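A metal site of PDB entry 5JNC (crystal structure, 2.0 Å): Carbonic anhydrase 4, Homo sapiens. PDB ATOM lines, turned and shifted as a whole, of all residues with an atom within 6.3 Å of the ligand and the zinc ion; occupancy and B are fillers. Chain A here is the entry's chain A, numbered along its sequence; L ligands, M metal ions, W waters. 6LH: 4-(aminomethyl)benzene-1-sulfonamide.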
ATOM      1  N   TYR A   7     -22.964  32.838   0.760  1.00  0.00           N
ATOM      2  CA  TYR A   7     -22.462  31.840  -0.192  1.00  0.00           C
ATOM      3  C   TYR A   7     -21.963  32.530  -1.486  1.00  0.00           C
ATOM      4  O   TYR A   7     -22.346  33.667  -1.788  1.00  0.00           O
ATOM      5  CB  TYR A   7     -23.555  30.797  -0.488  1.00  0.00           C
ATOM      6  CG  TYR A   7     -23.882  29.903   0.715  1.00  0.00           C
ATOM      7  CD1 TYR A   7     -22.971  28.936   1.173  1.00  0.00           C
ATOM      8  CD2 TYR A   7     -25.096  30.028   1.373  1.00  0.00           C
ATOM      9  CE1 TYR A   7     -23.295  28.122   2.269  1.00  0.00           C
ATOM     10  CE2 TYR A   7     -25.403  29.227   2.462  1.00  0.00           C
ATOM     11  CZ  TYR A   7     -24.519  28.282   2.906  1.00  0.00           C
ATOM     12  OH  TYR A   7     -24.905  27.511   3.966  1.00  0.00           O
ATOM     13  N   ASN A  68     -34.717  30.842   7.031  1.00  0.00           N
ATOM     14  CA  ASN A  68     -33.787  31.628   7.855  1.00  0.00           C
ATOM     15  C   ASN A  68     -32.833  32.532   7.083  1.00  0.00           C
ATOM     16  O   ASN A  68     -31.937  33.104   7.674  1.00  0.00           O
ATOM     17  CB  ASN A  68     -33.009  30.721   8.810  1.00  0.00           C
ATOM     18  CG  ASN A  68     -32.017  29.820   8.102  1.00  0.00           C
ATOM     19  OD1 ASN A  68     -31.736  29.973   6.930  1.00  0.00           O
ATOM     20  ND2 ASN A  68     -31.505  28.862   8.829  1.00  0.00           N
ATOM     21  N   HIS A  70     -30.718  31.487   4.613  1.00  0.00           N
ATOM     22  CA  HIS A  70     -29.747  30.641   3.881  1.00  0.00           C
ATOM     23  C   HIS A  70     -30.120  29.184   3.766  1.00  0.00           C
ATOM     24  O   HIS A  70     -29.327  28.406   3.238  1.00  0.00           O
ATOM     25  CB  HIS A  70     -28.332  30.779   4.489  1.00  0.00           C
ATOM     26  CG  HIS A  70     -28.343  30.940   5.958  1.00  0.00           C
ATOM     27  ND1 HIS A  70     -28.425  32.185   6.574  1.00  0.00           N
ATOM     28  CD2 HIS A  70     -28.286  30.024   6.962  1.00  0.00           C
ATOM     29  CE1 HIS A  70     -28.436  32.024   7.885  1.00  0.00           C
ATOM     30  NE2 HIS A  70     -28.344  30.721   8.147  1.00  0.00           N
ATOM     31  N   MET A  73     -35.714  25.498   7.337  1.00  0.00           N
ATOM     32  CA  MET A  73     -35.411  24.881   8.623  1.00  0.00           C
ATOM     33  C   MET A  73     -36.657  24.465   9.390  1.00  0.00           C
ATOM     34  O   MET A  73     -37.511  25.288   9.697  1.00  0.00           O
ATOM     35  CB  MET A  73     -34.601  25.859   9.436  1.00  0.00           C
ATOM     36  CG  MET A  73     -34.197  25.315  10.786  1.00  0.00           C
ATOM     37  SD  MET A  73     -33.065  26.455  11.630  1.00  0.00           S
ATOM     38  CE  MET A  73     -34.044  27.981  11.651  1.00  0.00           C
ATOM     39  N   GLN A  95     -33.072  20.915  15.038  1.00  0.00           N
ATOM     40  CA  GLN A  95     -33.559  21.393  13.752  1.00  0.00           C
ATOM     41  C   GLN A  95     -33.111  20.506  12.601  1.00  0.00           C
ATOM     42  O   GLN A  95     -32.111  19.781  12.699  1.00  0.00           O
ATOM     43  CB  GLN A  95     -33.149  22.833  13.516  1.00  0.00           C
ATOM     44  CG  GLN A  95     -31.687  23.155  13.803  1.00  0.00           C
ATOM     45  CD  GLN A  95     -30.867  23.556  12.587  1.00  0.00           C
ATOM     46  OE1 GLN A  95     -31.206  23.244  11.457  1.00  0.00           O
ATOM     47  NE2 GLN A  95     -29.776  24.237  12.828  1.00  0.00           N
ATOM     48  N   HIS A  97     -32.493  20.958   8.351  1.00  0.00           N
ATOM     49  CA  HIS A  97     -32.423  21.897   7.225  1.00  0.00           C
ATOM     50  C   HIS A  97     -31.748  21.248   6.030  1.00  0.00           C
ATOM     51  O   HIS A  97     -31.364  20.093   6.097  1.00  0.00           O
ATOM     52  CB  HIS A  97     -31.742  23.217   7.633  1.00  0.00           C
ATOM     53  CG  HIS A  97     -30.324  23.017   8.010  1.00  0.00           C
ATOM     54  ND1 HIS A  97     -29.934  22.781   9.303  1.00  0.00           N
ATOM     55  CD2 HIS A  97     -29.201  22.908   7.255  1.00  0.00           C
ATOM     56  CE1 HIS A  97     -28.634  22.574   9.352  1.00  0.00           C
ATOM     57  NE2 HIS A  97     -28.172  22.632   8.125  1.00  0.00           N
ATOM     58  N   LEU A  98     -31.685  21.967   4.904  1.00  0.00           N
ATOM     59  CA  LEU A  98     -31.118  21.420   3.668  1.00  0.00           C
ATOM     60  C   LEU A  98     -30.186  22.370   2.924  1.00  0.00           C
ATOM     61  O   LEU A  98     -30.130  23.566   3.153  1.00  0.00           O
ATOM     62  CB  LEU A  98     -32.233  20.917   2.733  1.00  0.00           C
ATOM     63  CG  LEU A  98     -33.218  19.870   3.265  1.00  0.00           C
ATOM     64  CD1 LEU A  98     -34.457  20.529   3.842  1.00  0.00           C
ATOM     65  CD2 LEU A  98     -33.668  18.900   2.185  1.00  0.00           C
ATOM     66  N   HIS A  99     -29.438  21.782   2.015  1.00  0.00           N
ATOM     67  CA  HIS A  99     -28.580  22.490   1.093  1.00  0.00           C
ATOM     68  C   HIS A  99     -28.883  21.903  -0.262  1.00  0.00           C
ATOM     69  O   HIS A  99     -29.068  20.673  -0.351  1.00  0.00           O
ATOM     70  CB  HIS A  99     -27.108  22.215   1.467  1.00  0.00           C
ATOM     71  CG  HIS A  99     -26.768  22.605   2.861  1.00  0.00           C
ATOM     72  ND1 HIS A  99     -26.221  23.837   3.166  1.00  0.00           N
ATOM     73  CD2 HIS A  99     -26.926  21.969   4.046  1.00  0.00           C
ATOM     74  CE1 HIS A  99     -26.018  23.925   4.468  1.00  0.00           C
ATOM     75  NE2 HIS A  99     -26.431  22.797   5.020  1.00  0.00           N
ATOM     76  N   GLU A 109     -23.205  18.952   0.303  1.00  0.00           N
ATOM     77  CA  GLU A 109     -22.068  19.611   0.902  1.00  0.00           C
ATOM     78  C   GLU A 109     -20.938  18.606   0.916  1.00  0.00           C
ATOM     79  O   GLU A 109     -19.849  18.894   0.398  1.00  0.00           O
ATOM     80  CB  GLU A 109     -22.414  20.170   2.311  1.00  0.00           C
ATOM     81  CG  GLU A 109     -23.348  21.366   2.263  1.00  0.00           C
ATOM     82  CD  GLU A 109     -23.146  22.331   3.425  1.00  0.00           C
ATOM     83  OE1 GLU A 109     -23.406  21.914   4.608  1.00  0.00           O
ATOM     84  OE2 GLU A 109     -22.734  23.497   3.159  1.00  0.00           O
ATOM     85  N   GLU A 120     -28.433  17.883   0.225  1.00  0.00           N
ATOM     86  CA  GLU A 120     -28.044  17.252   1.496  1.00  0.00           C
ATOM     87  C   GLU A 120     -28.893  17.771   2.643  1.00  0.00           C
ATOM     88  O   GLU A 120     -29.007  18.973   2.833  1.00  0.00           O
ATOM     89  CB  GLU A 120     -26.570  17.487   1.770  1.00  0.00           C
ATOM     90  CG  GLU A 120     -26.008  16.678   2.930  1.00  0.00           C
ATOM     91  CD  GLU A 120     -24.482  16.733   3.020  1.00  0.00           C
ATOM     92  OE1 GLU A 120     -23.773  16.848   1.995  1.00  0.00           O
ATOM     93  OE2 GLU A 120     -23.955  16.670   4.141  1.00  0.00           O
ATOM     94  N   MET A 121     -29.487  16.859   3.401  1.00  0.00           N
ATOM     95  CA  MET A 121     -30.338  17.194   4.555  1.00  0.00           C
ATOM     96  C   MET A 121     -29.569  16.926   5.825  1.00  0.00           C
ATOM     97  O   MET A 121     -28.954  15.852   5.981  1.00  0.00           O
ATOM     98  CB  MET A 121     -31.577  16.319   4.552  1.00  0.00           C
ATOM     99  CG  MET A 121     -32.584  16.614   5.650  1.00  0.00           C
ATOM    100  SD  MET A 121     -34.079  15.584   5.390  1.00  0.00           S
ATOM    101  CE  MET A 121     -33.468  14.131   6.132  1.00  0.00           C
ATOM    102  N   HIS A 122     -29.604  17.904   6.720  1.00  0.00           N
ATOM    103  CA  HIS A 122     -28.906  17.839   7.978  1.00  0.00           C
ATOM    104  C   HIS A 122     -29.927  17.879   9.085  1.00  0.00           C
ATOM    105  O   HIS A 122     -30.815  18.748   9.067  1.00  0.00           O
ATOM    106  CB  HIS A 122     -27.956  18.997   8.079  1.00  0.00           C
ATOM    107  CG  HIS A 122     -26.800  18.889   7.145  1.00  0.00           C
ATOM    108  ND1 HIS A 122     -26.067  19.972   6.749  1.00  0.00           N
ATOM    109  CD2 HIS A 122     -26.243  17.803   6.540  1.00  0.00           C
ATOM    110  CE1 HIS A 122     -25.090  19.568   5.947  1.00  0.00           C
ATOM    111  NE2 HIS A 122     -25.175  18.262   5.811  1.00  0.00           N
ATOM    112  N   ILE A 123     -29.859  16.902   9.991  1.00  0.00           N
ATOM    113  CA  ILE A 123     -30.643  16.917  11.198  1.00  0.00           C
ATOM    114  C   ILE A 123     -29.672  17.153  12.367  1.00  0.00           C
ATOM    115  O   ILE A 123     -28.749  16.357  12.621  1.00  0.00           O
ATOM    116  CB  ILE A 123     -31.477  15.627  11.399  1.00  0.00           C
ATOM    117  CG1 ILE A 123     -32.247  15.234  10.146  1.00  0.00           C
ATOM    118  CG2 ILE A 123     -32.502  15.831  12.505  1.00  0.00           C
ATOM    119  CD1 ILE A 123     -32.986  13.891  10.238  1.00  0.00           C
ATOM    120  N   VAL A 124     -29.921  18.234  13.095  1.00  0.00           N
ATOM    121  CA  VAL A 124     -28.984  18.776  14.033  1.00  0.00           C
ATOM    122  C   VAL A 124     -29.461  18.380  15.424  1.00  0.00           C
ATOM    123  O   VAL A 124     -30.606  18.634  15.785  1.00  0.00           O
ATOM    124  CB  VAL A 124     -28.883  20.301  13.891  1.00  0.00           C
ATOM    125  CG1 VAL A 124     -27.833  20.886  14.827  1.00  0.00           C
ATOM    126  CG2 VAL A 124     -28.521  20.672  12.471  1.00  0.00           C
ATOM    127  N   ILE A 145     -22.404  18.512  19.135  1.00  0.00           N
ATOM    128  CA  ILE A 145     -23.424  18.493  18.111  1.00  0.00           C
ATOM    129  C   ILE A 145     -23.239  17.235  17.290  1.00  0.00           C
ATOM    130  O   ILE A 145     -22.140  16.944  16.891  1.00  0.00           O
ATOM    131  CB  ILE A 145     -23.326  19.772  17.258  1.00  0.00           C
ATOM    132  CG1 ILE A 145     -23.656  20.961  18.158  1.00  0.00           C
ATOM    133  CG2 ILE A 145     -24.311  19.722  16.087  1.00  0.00           C
ATOM    134  CD1 ILE A 145     -23.613  22.284  17.479  1.00  0.00           C
ATOM    135  N   VAL A 147     -24.766  15.814  13.814  1.00  0.00           N
ATOM    136  CA  VAL A 147     -25.549  16.097  12.612  1.00  0.00           C
ATOM    137  C   VAL A 147     -25.621  14.804  11.853  1.00  0.00           C
ATOM    138  O   VAL A 147     -24.593  14.176  11.593  1.00  0.00           O
ATOM    139  CB  VAL A 147     -24.916  17.177  11.715  1.00  0.00           C
ATOM    140  CG1 VAL A 147     -25.740  17.350  10.454  1.00  0.00           C
ATOM    141  CG2 VAL A 147     -24.788  18.498  12.432  1.00  0.00           C
ATOM    142  N   SER A 205     -16.835  20.271  11.772  1.00  0.00           N
ATOM    143  CA  SER A 205     -17.417  21.533  12.138  1.00  0.00           C
ATOM    144  C   SER A 205     -18.820  21.691  11.574  1.00  0.00           C
ATOM    145  O   SER A 205     -19.278  20.925  10.734  1.00  0.00           O
ATOM    146  CB  SER A 205     -16.549  22.689  11.627  1.00  0.00           C
ATOM    147  OG  SER A 205     -16.685  22.887  10.244  1.00  0.00           O
ATOM    148  N   LEU A 206     -19.475  22.730  12.078  1.00  0.00           N
ATOM    149  CA  LEU A 206     -20.628  23.314  11.434  1.00  0.00           C
ATOM    150  C   LEU A 206     -20.173  23.947  10.117  1.00  0.00           C
ATOM    151  O   LEU A 206     -19.018  24.429   9.991  1.00  0.00           O
ATOM    152  CB  LEU A 206     -21.262  24.354  12.379  1.00  0.00           C
ATOM    153  CG  LEU A 206     -21.848  23.808  13.702  1.00  0.00           C
ATOM    154  CD1 LEU A 206     -22.125  24.899  14.719  1.00  0.00           C
ATOM    155  CD2 LEU A 206     -23.146  23.050  13.424  1.00  0.00           C
ATOM    156  N   THR A 207     -21.055  23.937   9.124  1.00  0.00           N
ATOM    157  CA  THR A 207     -20.734  24.427   7.789  1.00  0.00           C
ATOM    158  C   THR A 207     -21.199  25.838   7.473  1.00  0.00           C
ATOM    159  O   THR A 207     -21.164  26.263   6.308  1.00  0.00           O
ATOM    160  CB  THR A 207     -21.242  23.446   6.704  1.00  0.00           C
ATOM    161  OG1 THR A 207     -22.677  23.477   6.606  1.00  0.00           O
ATOM    162  CG2 THR A 207     -20.748  22.025   7.016  1.00  0.00           C
ATOM    163  N   THR A 208     -21.660  26.569   8.478  1.00  0.00           N
ATOM    164  CA  THR A 208     -21.825  28.010   8.345  1.00  0.00           C
ATOM    165  C   THR A 208     -21.152  28.700   9.535  1.00  0.00           C
ATOM    166  O   THR A 208     -20.956  28.093  10.579  1.00  0.00           O
ATOM    167  CB  THR A 208     -23.293  28.424   8.282  1.00  0.00           C
ATOM    168  OG1 THR A 208     -23.925  28.025   9.496  1.00  0.00           O
ATOM    169  CG2 THR A 208     -24.001  27.769   7.071  1.00  0.00           C
ATOM    170  N   PRO A 209     -20.769  29.977   9.355  1.00  0.00           N
ATOM    171  CA  PRO A 209     -20.119  30.724  10.457  1.00  0.00           C
ATOM    172  C   PRO A 209     -20.941  30.676  11.717  1.00  0.00           C
ATOM    173  O   PRO A 209     -22.150  30.729  11.616  1.00  0.00           O
ATOM    174  CB  PRO A 209     -20.013  32.132   9.892  1.00  0.00           C
ATOM    175  CG  PRO A 209     -19.860  31.891   8.417  1.00  0.00           C
ATOM    176  CD  PRO A 209     -20.814  30.776   8.120  1.00  0.00           C
ATOM    177  N   VAL A 215     -18.747  19.117  16.006  1.00  0.00           N
ATOM    178  CA  VAL A 215     -19.701  18.280  15.367  1.00  0.00           C
ATOM    179  C   VAL A 215     -19.157  16.866  15.156  1.00  0.00           C
ATOM    180  O   VAL A 215     -18.092  16.679  14.583  1.00  0.00           O
ATOM    181  CB  VAL A 215     -20.131  18.876  14.017  1.00  0.00           C
ATOM    182  CG1 VAL A 215     -21.137  17.952  13.333  1.00  0.00           C
ATOM    183  CG2 VAL A 215     -20.687  20.298  14.226  1.00  0.00           C
ATOM    184  N   TRP A 217     -20.035  14.006  12.856  1.00  0.00           N
ATOM    185  CA  TRP A 217     -20.734  13.850  11.586  1.00  0.00           C
ATOM    186  C   TRP A 217     -21.082  12.397  11.321  1.00  0.00           C
ATOM    187  O   TRP A 217     -20.279  11.491  11.555  1.00  0.00           O
ATOM    188  CB  TRP A 217     -19.867  14.382  10.422  1.00  0.00           C
ATOM    189  CG  TRP A 217     -19.988  15.813  10.279  1.00  0.00           C
ATOM    190  CD1 TRP A 217     -19.117  16.756  10.726  1.00  0.00           C
ATOM    191  CD2 TRP A 217     -21.079  16.514   9.700  1.00  0.00           C
ATOM    192  NE1 TRP A 217     -19.581  17.979  10.448  1.00  0.00           N
ATOM    193  CE2 TRP A 217     -20.785  17.875   9.806  1.00  0.00           C
ATOM    194  CE3 TRP A 217     -22.267  16.114   9.096  1.00  0.00           C
ATOM    195  CZ2 TRP A 217     -21.657  18.873   9.328  1.00  0.00           C
ATOM    196  CZ3 TRP A 217     -23.115  17.095   8.603  1.00  0.00           C
ATOM    197  CH2 TRP A 217     -22.813  18.457   8.715  1.00  0.00           C
HETATM  198  S1  6LH L   1     -24.725  22.492   9.525  1.00  0.00           S
HETATM  199  N1  6LH L   1     -27.259  27.579  12.823  1.00  0.00           N
HETATM  200  C10 6LH L   1     -26.178  26.771  13.402  1.00  0.00           C
HETATM  201  C11 6LH L   1     -25.815  25.686  12.421  1.00  0.00           C
HETATM  202  N2  6LH L   1     -24.900  22.968   8.054  1.00  0.00           N
HETATM  203  O5  6LH L   1     -25.492  21.280   9.834  1.00  0.00           O
HETATM  204  C12 6LH L   1     -26.388  24.421  12.537  1.00  0.00           C
HETATM  205  O6  6LH L   1     -23.322  22.156   9.758  1.00  0.00           O
HETATM  206  C13 6LH L   1     -26.051  23.423  11.622  1.00  0.00           C
HETATM  207  C14 6LH L   1     -25.154  23.667  10.576  1.00  0.00           C
HETATM  208  C15 6LH L   1     -24.610  24.941  10.464  1.00  0.00           C
HETATM  209  C16 6LH L   1     -24.935  25.933  11.397  1.00  0.00           C
HETATM  210 ZN    ZN M   1     -26.321  22.109   7.087  1.00  0.00          ZN
HETATM  211  O   HOH W   1     -22.955  27.819  12.825  1.00  0.00           O
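NE2 of His 122 is in hydrogen-bond range of OE2 of Glu 120, 2.6 Å away.
NE2 of His 99 lies close to OE1 of Glu 109 (3.2 Å).
N of Glu 120 sits at hydrogen-bond distance from O of His 99, 2.9 Å away.
OG1 of Thr 207 is in hydrogen-bond range of OE1 of Glu 109, 2.6 Å away.
The backbone carbonyl oxygen (O) of Gln 95 lies within hydrogen-bond range of the backbone NH (N) of Val 124 (2.7 Å).
OE1 of Gln 95 lies close to SD of Met 73.
O of Ser 205 lies within hydrogen-bond range of NE1 of Trp 217.
OE1 of Glu 120 is in hydrogen-bond range of N of Glu 109 (2.8 Å).
Glu 109 touches the zinc ion (OE1 to ZN, 3.8 Å).
OG1 of Thr 207 touches the zinc ion, 3.9 Å away.
Along chain A the residues within 4 Å of the zinc ion span positions 97 to 207.
O6 of the ligand sits at hydrogen-bond distance from N of Thr 207 (3.0 Å).
An oxygen (O6) of the ligand sits at hydrogen-bond distance from the side-chain hydroxyl (OG1) of Thr 207 (3.5 Å).
Merely in contact with the ligand: Thr 208 (3.0 Å), Leu 206 (3.4 Å), Gln 95 (3.4 Å), Trp 217 (3.7 Å), Val 124 (3.8 Å), Val 147 (3.9 Å) and Glu 109 (3.9 Å).
Hydrophobic or aromatic side chains within 4 Å of the ligand: His 97, His 99, His 122, Val 124, Val 147, Leu 206 and Trp 217.
Of the 23 residues printed, 11 come within 4 Å of the ligand.
Along chain A the residues within 4 Å of the ligand span positions 95 to 217.
The nearest printed residue that does not touch the ligand is Ser 205 (4.3 Å).
The zinc ion is bound by N2 of the ligand (1.9 Å), ND1 of His 122 (2.2 Å), NE2 of His 99 (2.2 Å) and NE2 of His 97 (2.2 Å).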
